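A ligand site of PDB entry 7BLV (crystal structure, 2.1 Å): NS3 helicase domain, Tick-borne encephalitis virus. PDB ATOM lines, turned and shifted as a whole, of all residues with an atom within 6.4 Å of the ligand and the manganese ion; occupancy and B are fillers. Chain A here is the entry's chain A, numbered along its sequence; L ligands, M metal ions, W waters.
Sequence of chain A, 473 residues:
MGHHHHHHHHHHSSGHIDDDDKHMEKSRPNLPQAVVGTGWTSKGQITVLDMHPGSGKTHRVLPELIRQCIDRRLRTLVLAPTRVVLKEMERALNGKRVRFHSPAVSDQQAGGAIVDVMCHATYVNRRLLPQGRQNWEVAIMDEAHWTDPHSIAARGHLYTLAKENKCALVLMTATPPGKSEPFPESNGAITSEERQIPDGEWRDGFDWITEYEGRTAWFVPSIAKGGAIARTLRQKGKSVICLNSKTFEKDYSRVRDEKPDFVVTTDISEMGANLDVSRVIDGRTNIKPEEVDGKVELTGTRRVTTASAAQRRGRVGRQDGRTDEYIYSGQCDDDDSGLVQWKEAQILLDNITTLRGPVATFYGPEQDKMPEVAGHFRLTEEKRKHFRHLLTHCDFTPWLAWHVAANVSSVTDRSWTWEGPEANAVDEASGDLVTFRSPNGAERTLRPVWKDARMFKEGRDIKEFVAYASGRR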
ATOM      1  N   MET A  51      34.017 -12.457 -25.367  1.00  0.00           N
ATOM      2  CA  MET A  51      33.327 -13.502 -26.096  1.00  0.00           C
ATOM      3  C   MET A  51      33.081 -13.004 -27.511  1.00  0.00           C
ATOM      4  O   MET A  51      32.887 -11.803 -27.718  1.00  0.00           O
ATOM      5  CB  MET A  51      31.992 -13.849 -25.401  1.00  0.00           C
ATOM      6  CG  MET A  51      32.048 -13.747 -23.875  1.00  0.00           C
ATOM      7  SD  MET A  51      32.985 -15.099 -23.033  1.00  0.00           S
ATOM      8  CE  MET A  51      34.532 -14.259 -22.539  1.00  0.00           C
ATOM      9  N   HIS A  52      33.128 -13.925 -28.501  1.00  0.00           N
ATOM     10  CA  HIS A  52      32.980 -13.555 -29.908  1.00  0.00           C
ATOM     11  C   HIS A  52      31.677 -12.760 -30.111  1.00  0.00           C
ATOM     12  O   HIS A  52      30.802 -12.740 -29.233  1.00  0.00           O
ATOM     13  CB  HIS A  52      33.179 -14.784 -30.823  1.00  0.00           C
ATOM     14  CG  HIS A  52      32.083 -15.802 -30.762  1.00  0.00           C
ATOM     15  ND1 HIS A  52      30.839 -15.598 -31.355  1.00  0.00           N
ATOM     16  CD2 HIS A  52      32.034 -17.030 -30.187  1.00  0.00           C
ATOM     17  CE1 HIS A  52      30.082 -16.647 -31.136  1.00  0.00           C
ATOM     18  NE2 HIS A  52      30.790 -17.542 -30.425  1.00  0.00           N
ATOM     19  N   PRO A  53      31.504 -12.047 -31.253  1.00  0.00           N
ATOM     20  CA  PRO A  53      30.247 -11.298 -31.500  1.00  0.00           C
ATOM     21  C   PRO A  53      29.017 -12.204 -31.520  1.00  0.00           C
ATOM     22  O   PRO A  53      29.091 -13.358 -31.953  1.00  0.00           O
ATOM     23  CB  PRO A  53      30.471 -10.645 -32.883  1.00  0.00           C
ATOM     24  CG  PRO A  53      31.992 -10.663 -33.089  1.00  0.00           C
ATOM     25  CD  PRO A  53      32.496 -11.887 -32.349  1.00  0.00           C
ATOM     26  N   GLY A  54      27.880 -11.681 -31.024  1.00  0.00           N
ATOM     27  CA  GLY A  54      26.630 -12.439 -30.926  1.00  0.00           C
ATOM     28  C   GLY A  54      26.674 -13.549 -29.864  1.00  0.00           C
ATOM     29  O   GLY A  54      25.711 -14.310 -29.760  1.00  0.00           O
ATOM     30  N   SER A  55      27.763 -13.641 -29.069  1.00  0.00           N
ATOM     31  CA  SER A  55      27.889 -14.579 -27.950  1.00  0.00           C
ATOM     32  C   SER A  55      26.696 -14.527 -26.985  1.00  0.00           C
ATOM     33  O   SER A  55      26.237 -15.566 -26.500  1.00  0.00           O
ATOM     34  CB  SER A  55      29.180 -14.402 -27.195  1.00  0.00           C
ATOM     35  OG  SER A  55      30.237 -15.130 -27.819  1.00  0.00           O
ATOM     36  N   GLY A  56      26.187 -13.327 -26.702  1.00  0.00           N
ATOM     37  CA  GLY A  56      25.035 -13.164 -25.802  1.00  0.00           C
ATOM     38  C   GLY A  56      25.356 -12.207 -24.653  1.00  0.00           C
ATOM     39  O   GLY A  56      24.632 -12.141 -23.672  1.00  0.00           O
ATOM     40  N   LYS A  57      26.463 -11.457 -24.825  1.00  0.00           N
ATOM     41  CA  LYS A  57      26.991 -10.505 -23.858  1.00  0.00           C
ATOM     42  C   LYS A  57      25.892  -9.535 -23.423  1.00  0.00           C
ATOM     43  O   LYS A  57      25.651  -9.370 -22.230  1.00  0.00           O
ATOM     44  CB  LYS A  57      28.225  -9.808 -24.434  1.00  0.00           C
ATOM     45  CG  LYS A  57      29.430 -10.718 -24.593  1.00  0.00           C
ATOM     46  CD  LYS A  57      30.695 -10.011 -25.043  1.00  0.00           C
ATOM     47  CE  LYS A  57      30.822  -9.976 -26.620  1.00  0.00           C
ATOM     48  NZ  LYS A  57      30.549 -11.362 -27.092  1.00  0.00           N
ATOM     49  N   THR A  58      25.205  -8.945 -24.401  1.00  0.00           N
ATOM     50  CA  THR A  58      24.182  -7.946 -24.097  1.00  0.00           C
ATOM     51  C   THR A  58      22.874  -8.616 -23.632  1.00  0.00           C
ATOM     52  O   THR A  58      22.240  -8.155 -22.689  1.00  0.00           O
ATOM     53  CB  THR A  58      24.035  -6.909 -25.229  1.00  0.00           C
ATOM     54  OG1 THR A  58      25.330  -6.426 -25.602  1.00  0.00           O
ATOM     55  CG2 THR A  58      23.170  -5.715 -24.859  1.00  0.00           C
ATOM     56  N   HIS A  59      22.455  -9.694 -24.293  1.00  0.00           N
ATOM     57  CA  HIS A  59      21.089 -10.120 -24.041  1.00  0.00           C
ATOM     58  C   HIS A  59      21.002 -11.221 -22.973  1.00  0.00           C
ATOM     59  O   HIS A  59      19.967 -11.360 -22.321  1.00  0.00           O
ATOM     60  CB  HIS A  59      20.291 -10.355 -25.347  1.00  0.00           C
ATOM     61  CG  HIS A  59      18.936  -9.687 -25.322  1.00  0.00           C
ATOM     62  ND1 HIS A  59      17.879 -10.169 -24.536  1.00  0.00           N
ATOM     63  CD2 HIS A  59      18.477  -8.575 -25.935  1.00  0.00           C
ATOM     64  CE1 HIS A  59      16.802  -9.412 -24.685  1.00  0.00           C
ATOM     65  NE2 HIS A  59      17.152  -8.416 -25.546  1.00  0.00           N
ATOM     66  N   ARG A  60      22.106 -11.964 -22.773  1.00  0.00           N
ATOM     67  CA  ARG A  60      22.106 -13.089 -21.837  1.00  0.00           C
ATOM     68  C   ARG A  60      22.965 -12.800 -20.597  1.00  0.00           C
ATOM     69  O   ARG A  60      22.459 -12.826 -19.481  1.00  0.00           O
ATOM     70  CB  ARG A  60      22.627 -14.341 -22.557  1.00  0.00           C
ATOM     71  CG  ARG A  60      22.186 -15.662 -21.902  1.00  0.00           C
ATOM     72  CD  ARG A  60      22.729 -16.855 -22.703  1.00  0.00           C
ATOM     73  NE  ARG A  60      24.093 -16.676 -23.212  1.00  0.00           N
ATOM     74  CZ  ARG A  60      25.209 -17.089 -22.603  1.00  0.00           C
ATOM     75  NH1 ARG A  60      25.146 -17.728 -21.454  1.00  0.00           N
ATOM     76  NH2 ARG A  60      26.396 -16.860 -23.165  1.00  0.00           N
ATOM     77  N   VAL A  61      24.259 -12.528 -20.825  1.00  0.00           N
ATOM     78  CA  VAL A  61      25.266 -12.395 -19.795  1.00  0.00           C
ATOM     79  C   VAL A  61      24.974 -11.201 -18.876  1.00  0.00           C
ATOM     80  O   VAL A  61      25.070 -11.297 -17.650  1.00  0.00           O
ATOM     81  CB  VAL A  61      26.674 -12.305 -20.418  1.00  0.00           C
ATOM     82  CG1 VAL A  61      27.722 -11.853 -19.406  1.00  0.00           C
ATOM     83  CG2 VAL A  61      27.095 -13.608 -21.088  1.00  0.00           C
ATOM     84  N   GLU A  88      17.162  -1.019 -25.391  1.00  0.00           N
ATOM     85  CA  GLU A  88      17.068  -2.470 -25.508  1.00  0.00           C
ATOM     86  C   GLU A  88      17.489  -3.169 -24.210  1.00  0.00           C
ATOM     87  O   GLU A  88      17.050  -4.280 -23.942  1.00  0.00           O
ATOM     88  CB  GLU A  88      17.837  -2.975 -26.730  1.00  0.00           C
ATOM     89  CG  GLU A  88      17.444  -4.394 -27.128  1.00  0.00           C
ATOM     90  CD  GLU A  88      17.608  -4.786 -28.601  1.00  0.00           C
ATOM     91  OE1 GLU A  88      17.906  -3.873 -29.440  1.00  0.00           O
ATOM     92  OE2 GLU A  88      17.441  -5.992 -28.911  1.00  0.00           O
ATOM     93  N   ASP A 142      29.382  -2.119 -21.501  1.00  0.00           N
ATOM     94  CA  ASP A 142      29.051  -2.788 -22.746  1.00  0.00           C
ATOM     95  C   ASP A 142      29.655  -2.066 -23.959  1.00  0.00           C
ATOM     96  O   ASP A 142      29.841  -0.836 -23.972  1.00  0.00           O
ATOM     97  CB  ASP A 142      27.535  -2.871 -22.886  1.00  0.00           C
ATOM     98  CG  ASP A 142      26.974  -3.956 -23.813  1.00  0.00           C
ATOM     99  OD1 ASP A 142      27.685  -4.902 -24.068  1.00  0.00           O
ATOM    100  OD2 ASP A 142      25.811  -3.817 -24.250  1.00  0.00           O
ATOM    101  N   GLU A 143      29.956  -2.859 -24.990  1.00  0.00           N
ATOM    102  CA  GLU A 143      30.573  -2.405 -26.228  1.00  0.00           C
ATOM    103  C   GLU A 143      31.744  -1.498 -25.907  1.00  0.00           C
ATOM    104  O   GLU A 143      31.805  -0.404 -26.447  1.00  0.00           O
ATOM    105  CB  GLU A 143      29.597  -1.616 -27.130  1.00  0.00           C
ATOM    106  CG  GLU A 143      28.292  -2.295 -27.412  1.00  0.00           C
ATOM    107  CD  GLU A 143      28.414  -3.628 -28.141  1.00  0.00           C
ATOM    108  OE1 GLU A 143      29.500  -3.925 -28.622  1.00  0.00           O
ATOM    109  OE2 GLU A 143      27.423  -4.347 -28.223  1.00  0.00           O
ATOM    110  N   MET A 172      32.762  -5.653 -21.498  1.00  0.00           N
ATOM    111  CA  MET A 172      32.168  -6.604 -22.419  1.00  0.00           C
ATOM    112  C   MET A 172      32.382  -6.114 -23.865  1.00  0.00           C
ATOM    113  O   MET A 172      31.745  -5.118 -24.265  1.00  0.00           O
ATOM    114  CB  MET A 172      30.670  -6.645 -22.180  1.00  0.00           C
ATOM    115  CG  MET A 172      30.279  -6.877 -20.741  1.00  0.00           C
ATOM    116  SD  MET A 172      28.635  -7.672 -20.688  1.00  0.00           S
ATOM    117  CE  MET A 172      27.529  -6.366 -21.223  1.00  0.00           C
ATOM    118  N   ALA A 174      33.488  -7.982 -27.988  1.00  0.00           N
ATOM    119  CA  ALA A 174      34.080  -8.908 -28.937  1.00  0.00           C
ATOM    120  C   ALA A 174      35.540  -8.557 -29.208  1.00  0.00           C
ATOM    121  O   ALA A 174      36.355  -9.437 -29.455  1.00  0.00           O
ATOM    122  CB  ALA A 174      33.207  -8.869 -30.182  1.00  0.00           C
ATOM    123  N   ASN A 187      28.188 -17.045 -34.528  1.00  0.00           N
ATOM    124  CA  ASN A 187      27.121 -18.001 -34.242  1.00  0.00           C
ATOM    125  C   ASN A 187      26.806 -18.874 -35.449  1.00  0.00           C
ATOM    126  O   ASN A 187      26.322 -19.997 -35.298  1.00  0.00           O
ATOM    127  CB  ASN A 187      25.809 -17.316 -33.847  1.00  0.00           C
ATOM    128  CG  ASN A 187      25.893 -16.624 -32.505  1.00  0.00           C
ATOM    129  OD1 ASN A 187      26.865 -16.814 -31.772  1.00  0.00           O
ATOM    130  ND2 ASN A 187      24.899 -15.803 -32.170  1.00  0.00           N
ATOM    131  N   GLY A 272      26.783  -2.590 -31.502  1.00  0.00           N
ATOM    132  CA  GLY A 272      25.608  -3.339 -31.041  1.00  0.00           C
ATOM    133  C   GLY A 272      24.338  -3.206 -31.887  1.00  0.00           C
ATOM    134  O   GLY A 272      23.298  -3.774 -31.526  1.00  0.00           O
ATOM    135  N   ASN A 274      21.734  -4.310 -34.631  1.00  0.00           N
ATOM    136  CA  ASN A 274      21.303  -5.527 -35.311  1.00  0.00           C
ATOM    137  C   ASN A 274      20.540  -5.105 -36.557  1.00  0.00           C
ATOM    138  O   ASN A 274      19.381  -4.703 -36.479  1.00  0.00           O
ATOM    139  CB  ASN A 274      20.336  -6.399 -34.483  1.00  0.00           C
ATOM    140  CG  ASN A 274      19.700  -7.537 -35.282  1.00  0.00           C
ATOM    141  OD1 ASN A 274      20.328  -8.142 -36.176  1.00  0.00           O
ATOM    142  ND2 ASN A 274      18.438  -7.848 -34.974  1.00  0.00           N
ATOM    143  N   ARG A 318      25.158 -13.978 -37.179  1.00  0.00           N
ATOM    144  CA  ARG A 318      24.609 -13.884 -35.842  1.00  0.00           C
ATOM    145  C   ARG A 318      23.619 -15.032 -35.569  1.00  0.00           C
ATOM    146  O   ARG A 318      23.189 -15.201 -34.419  1.00  0.00           O
ATOM    147  CB  ARG A 318      23.954 -12.516 -35.627  1.00  0.00           C
ATOM    148  CG  ARG A 318      24.940 -11.342 -35.497  1.00  0.00           C
ATOM    149  CD  ARG A 318      24.263  -9.970 -35.466  1.00  0.00           C
ATOM    150  NE  ARG A 318      23.740  -9.639 -34.142  1.00  0.00           N
ATOM    151  CZ  ARG A 318      22.503  -9.904 -33.710  1.00  0.00           C
ATOM    152  NH1 ARG A 318      21.623 -10.513 -34.496  1.00  0.00           N
ATOM    153  NH2 ARG A 318      22.139  -9.564 -32.481  1.00  0.00           N
ATOM    154  N   GLN A 319      23.278 -15.820 -36.607  1.00  0.00           N
ATOM    155  CA  GLN A 319      22.277 -16.867 -36.484  1.00  0.00           C
ATOM    156  C   GLN A 319      22.877 -18.239 -36.808  1.00  0.00           C
ATOM    157  O   GLN A 319      23.520 -18.441 -37.837  1.00  0.00           O
ATOM    158  CB  GLN A 319      21.066 -16.508 -37.359  1.00  0.00           C
ATOM    159  CG  GLN A 319      19.791 -17.302 -37.029  1.00  0.00           C
ATOM    160  CD  GLN A 319      18.733 -17.130 -38.091  1.00  0.00           C
ATOM    161  OE1 GLN A 319      18.577 -16.043 -38.669  1.00  0.00           O
ATOM    162  NE2 GLN A 319      17.989 -18.195 -38.385  1.00  0.00           N
ATOM    163  N   ASP A 320      22.661 -19.187 -35.908  1.00  0.00           N
ATOM    164  CA  ASP A 320      22.974 -20.607 -36.094  1.00  0.00           C
ATOM    165  C   ASP A 320      22.202 -21.195 -37.300  1.00  0.00           C
ATOM    166  O   ASP A 320      20.969 -21.020 -37.417  1.00  0.00           O
ATOM    167  CB  ASP A 320      22.616 -21.333 -34.794  1.00  0.00           C
ATOM    168  CG  ASP A 320      22.726 -22.849 -34.860  1.00  0.00           C
ATOM    169  OD1 ASP A 320      23.841 -23.336 -35.190  1.00  0.00           O
ATOM    170  OD2 ASP A 320      21.684 -23.519 -34.582  1.00  0.00           O
HETATM  171  P1  LIG L   1      26.855 -10.060 -28.134  1.00  0.00           P
HETATM  172  O1  LIG L   1      27.248  -9.561 -29.524  1.00  0.00           O
HETATM  173  O2  LIG L   1      27.925 -10.971 -27.575  1.00  0.00           O
HETATM  174  O3  LIG L   1      26.507  -8.957 -27.190  1.00  0.00           O
HETATM  175  P2  LIG L   1      23.937 -10.505 -27.942  1.00  0.00           P
HETATM  176  O4  LIG L   1      23.535  -9.318 -28.755  1.00  0.00           O
HETATM  177  O5  LIG L   1      23.745 -10.410 -26.467  1.00  0.00           O
HETATM  178  O6  LIG L   1      25.466 -10.870 -28.296  1.00  0.00           O
HETATM  179  O7  LIG L   1      23.162 -11.795 -28.470  1.00  0.00           O
HETATM  180  C1  LIG L   1      23.325 -12.159 -29.889  1.00  0.00           C
HETATM  181  C2  LIG L   1      22.440 -13.404 -30.050  1.00  0.00           C
HETATM  182  O8  LIG L   1      21.166 -13.194 -29.357  1.00  0.00           O
HETATM  183  C3  LIG L   1      22.094 -13.779 -31.501  1.00  0.00           C
HETATM  184  O9  LIG L   1      22.227 -15.179 -31.688  1.00  0.00           O
HETATM  185  C4  LIG L   1      20.638 -13.320 -31.616  1.00  0.00           C
HETATM  186  O10 LIG L   1      19.932 -14.013 -32.633  1.00  0.00           O
HETATM  187  C5  LIG L   1      20.142 -13.660 -30.214  1.00  0.00           C
HETATM  188  N1  LIG L   1      18.871 -13.046 -29.835  1.00  0.00           N
HETATM  189  C6  LIG L   1      17.689 -13.714 -29.623  1.00  0.00           C
HETATM  190  N2  LIG L   1      16.688 -12.916 -29.302  1.00  0.00           N
HETATM  191  C7  LIG L   1      17.248 -11.639 -29.308  1.00  0.00           C
HETATM  192  C8  LIG L   1      16.702 -10.357 -29.044  1.00  0.00           C
HETATM  193  N3  LIG L   1      15.420 -10.158 -28.719  1.00  0.00           N
HETATM  194  N4  LIG L   1      17.539  -9.291 -29.145  1.00  0.00           N
HETATM  195  C9  LIG L   1      18.816  -9.503 -29.478  1.00  0.00           C
HETATM  196  N5  LIG L   1      19.438 -10.658 -29.735  1.00  0.00           N
HETATM  197  C10 LIG L   1      18.600 -11.703 -29.641  1.00  0.00           C
HETATM  198 MN    MN M   1      26.960  -6.702 -27.468  1.00  0.00          MN
HETATM  199  O   HOH W   1      24.942  -6.232 -28.114  1.00  0.00           O
HETATM  200  O   HOH W   2      29.031  -7.518 -26.777  1.00  0.00           O
HETATM  201  O   HOH W   3      28.867  -7.533 -29.823  1.00  0.00           O
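The side-chain amino group of Lys 57 is in salt-bridge range of an oxygen (O2) of the ligand (2.7 Å). N of Gly 56 is in hydrogen-bond range of O6 of the ligand. The backbone NH (N) of Lys 57 lies within hydrogen-bond range of an oxygen (O2) of the ligand, 3.2 Å away. The backbone NH (N) of Gly 54 lies within hydrogen-bond range of an oxygen (O1) of the ligand (2.7 Å). The backbone carbonyl oxygen (O) of Arg 318 is in hydrogen-bond range of an oxygen (O9) of the ligand (2.9 Å). N of His 59 is in hydrogen-bond range of O5 of the ligand (2.6 Å). An oxygen (O5) of the ligand sits at hydrogen-bond distance from the backbone NH (N) of Thr 58 (2.9 Å). The backbone NH (N) of Ser 55 sits at hydrogen-bond distance from an oxygen (O2) of the ligand (3.1 Å). The guanidinium group of Arg 318 lies within salt-bridge range of an oxygen (O4) of the ligand, at 3.99 Å. The side-chain amide nitrogen of Asn 187 sits at hydrogen-bond distance from an oxygen (O9) of the ligand (2.8 Å).
Asp 142 touches the manganese ion (OD1 to MN, 3.9 Å). Three residues have an atom within 4 Å of the manganese ion: Thr 58, Asp 142 and Glu 143. The nearest printed residue that does not touch the manganese ion is Lys 57 (4.5 Å).
OE2 of Glu 88 lies close to N4 of the ligand, at 3.3 Å. Merely in contact with the ligand: Pro 53 (3.8 Å) and His 52 (3.8 Å). The nearest printed residue that does not touch the ligand is Arg 60 (4.3 Å).
The side-chain amino group (NZ) of Lys 57 lies within hydrogen-bond range of the backbone carbonyl oxygen (O) of His 52. The backbone carbonyl oxygen (O) of Arg 318 is in hydrogen-bond range of the side-chain amide nitrogen (ND2) of Asn 187. N of Val 61 lies within hydrogen-bond range of O of Gly 56 (2.9 Å). The backbone carbonyl oxygen (O) of His 52 sits at hydrogen-bond distance from the side-chain hydroxyl (OG) of Ser 55 (2.8 Å). The backbone carbonyl oxygen (O) of Gly 54 is in hydrogen-bond range of the side-chain amide nitrogen (ND2) of Asn 187 (2.9 Å). The side-chain amide oxygen (OD1) of Asn 274 lies within hydrogen-bond range of the guanidinium group (NH1) of Arg 318 (3.2 Å). The backbone carbonyl oxygen (O) of Met 51 lies within hydrogen-bond range of the side-chain amino group (NZ) of Lys 57. The backbone NH (N) of Glu 143 is in hydrogen-bond range of the backbone carbonyl oxygen (O) of Met 172.
The manganese ion is bound by water W1 (2.2 Å), an oxygen (O3) of the ligand (2.3 Å), water W2 (2.3 Å), the side-chain hydroxyl (OG1) of Thr 58 (2.5 Å) and the side-chain carboxylate (OE2) of Glu 143 (2.5 Å).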
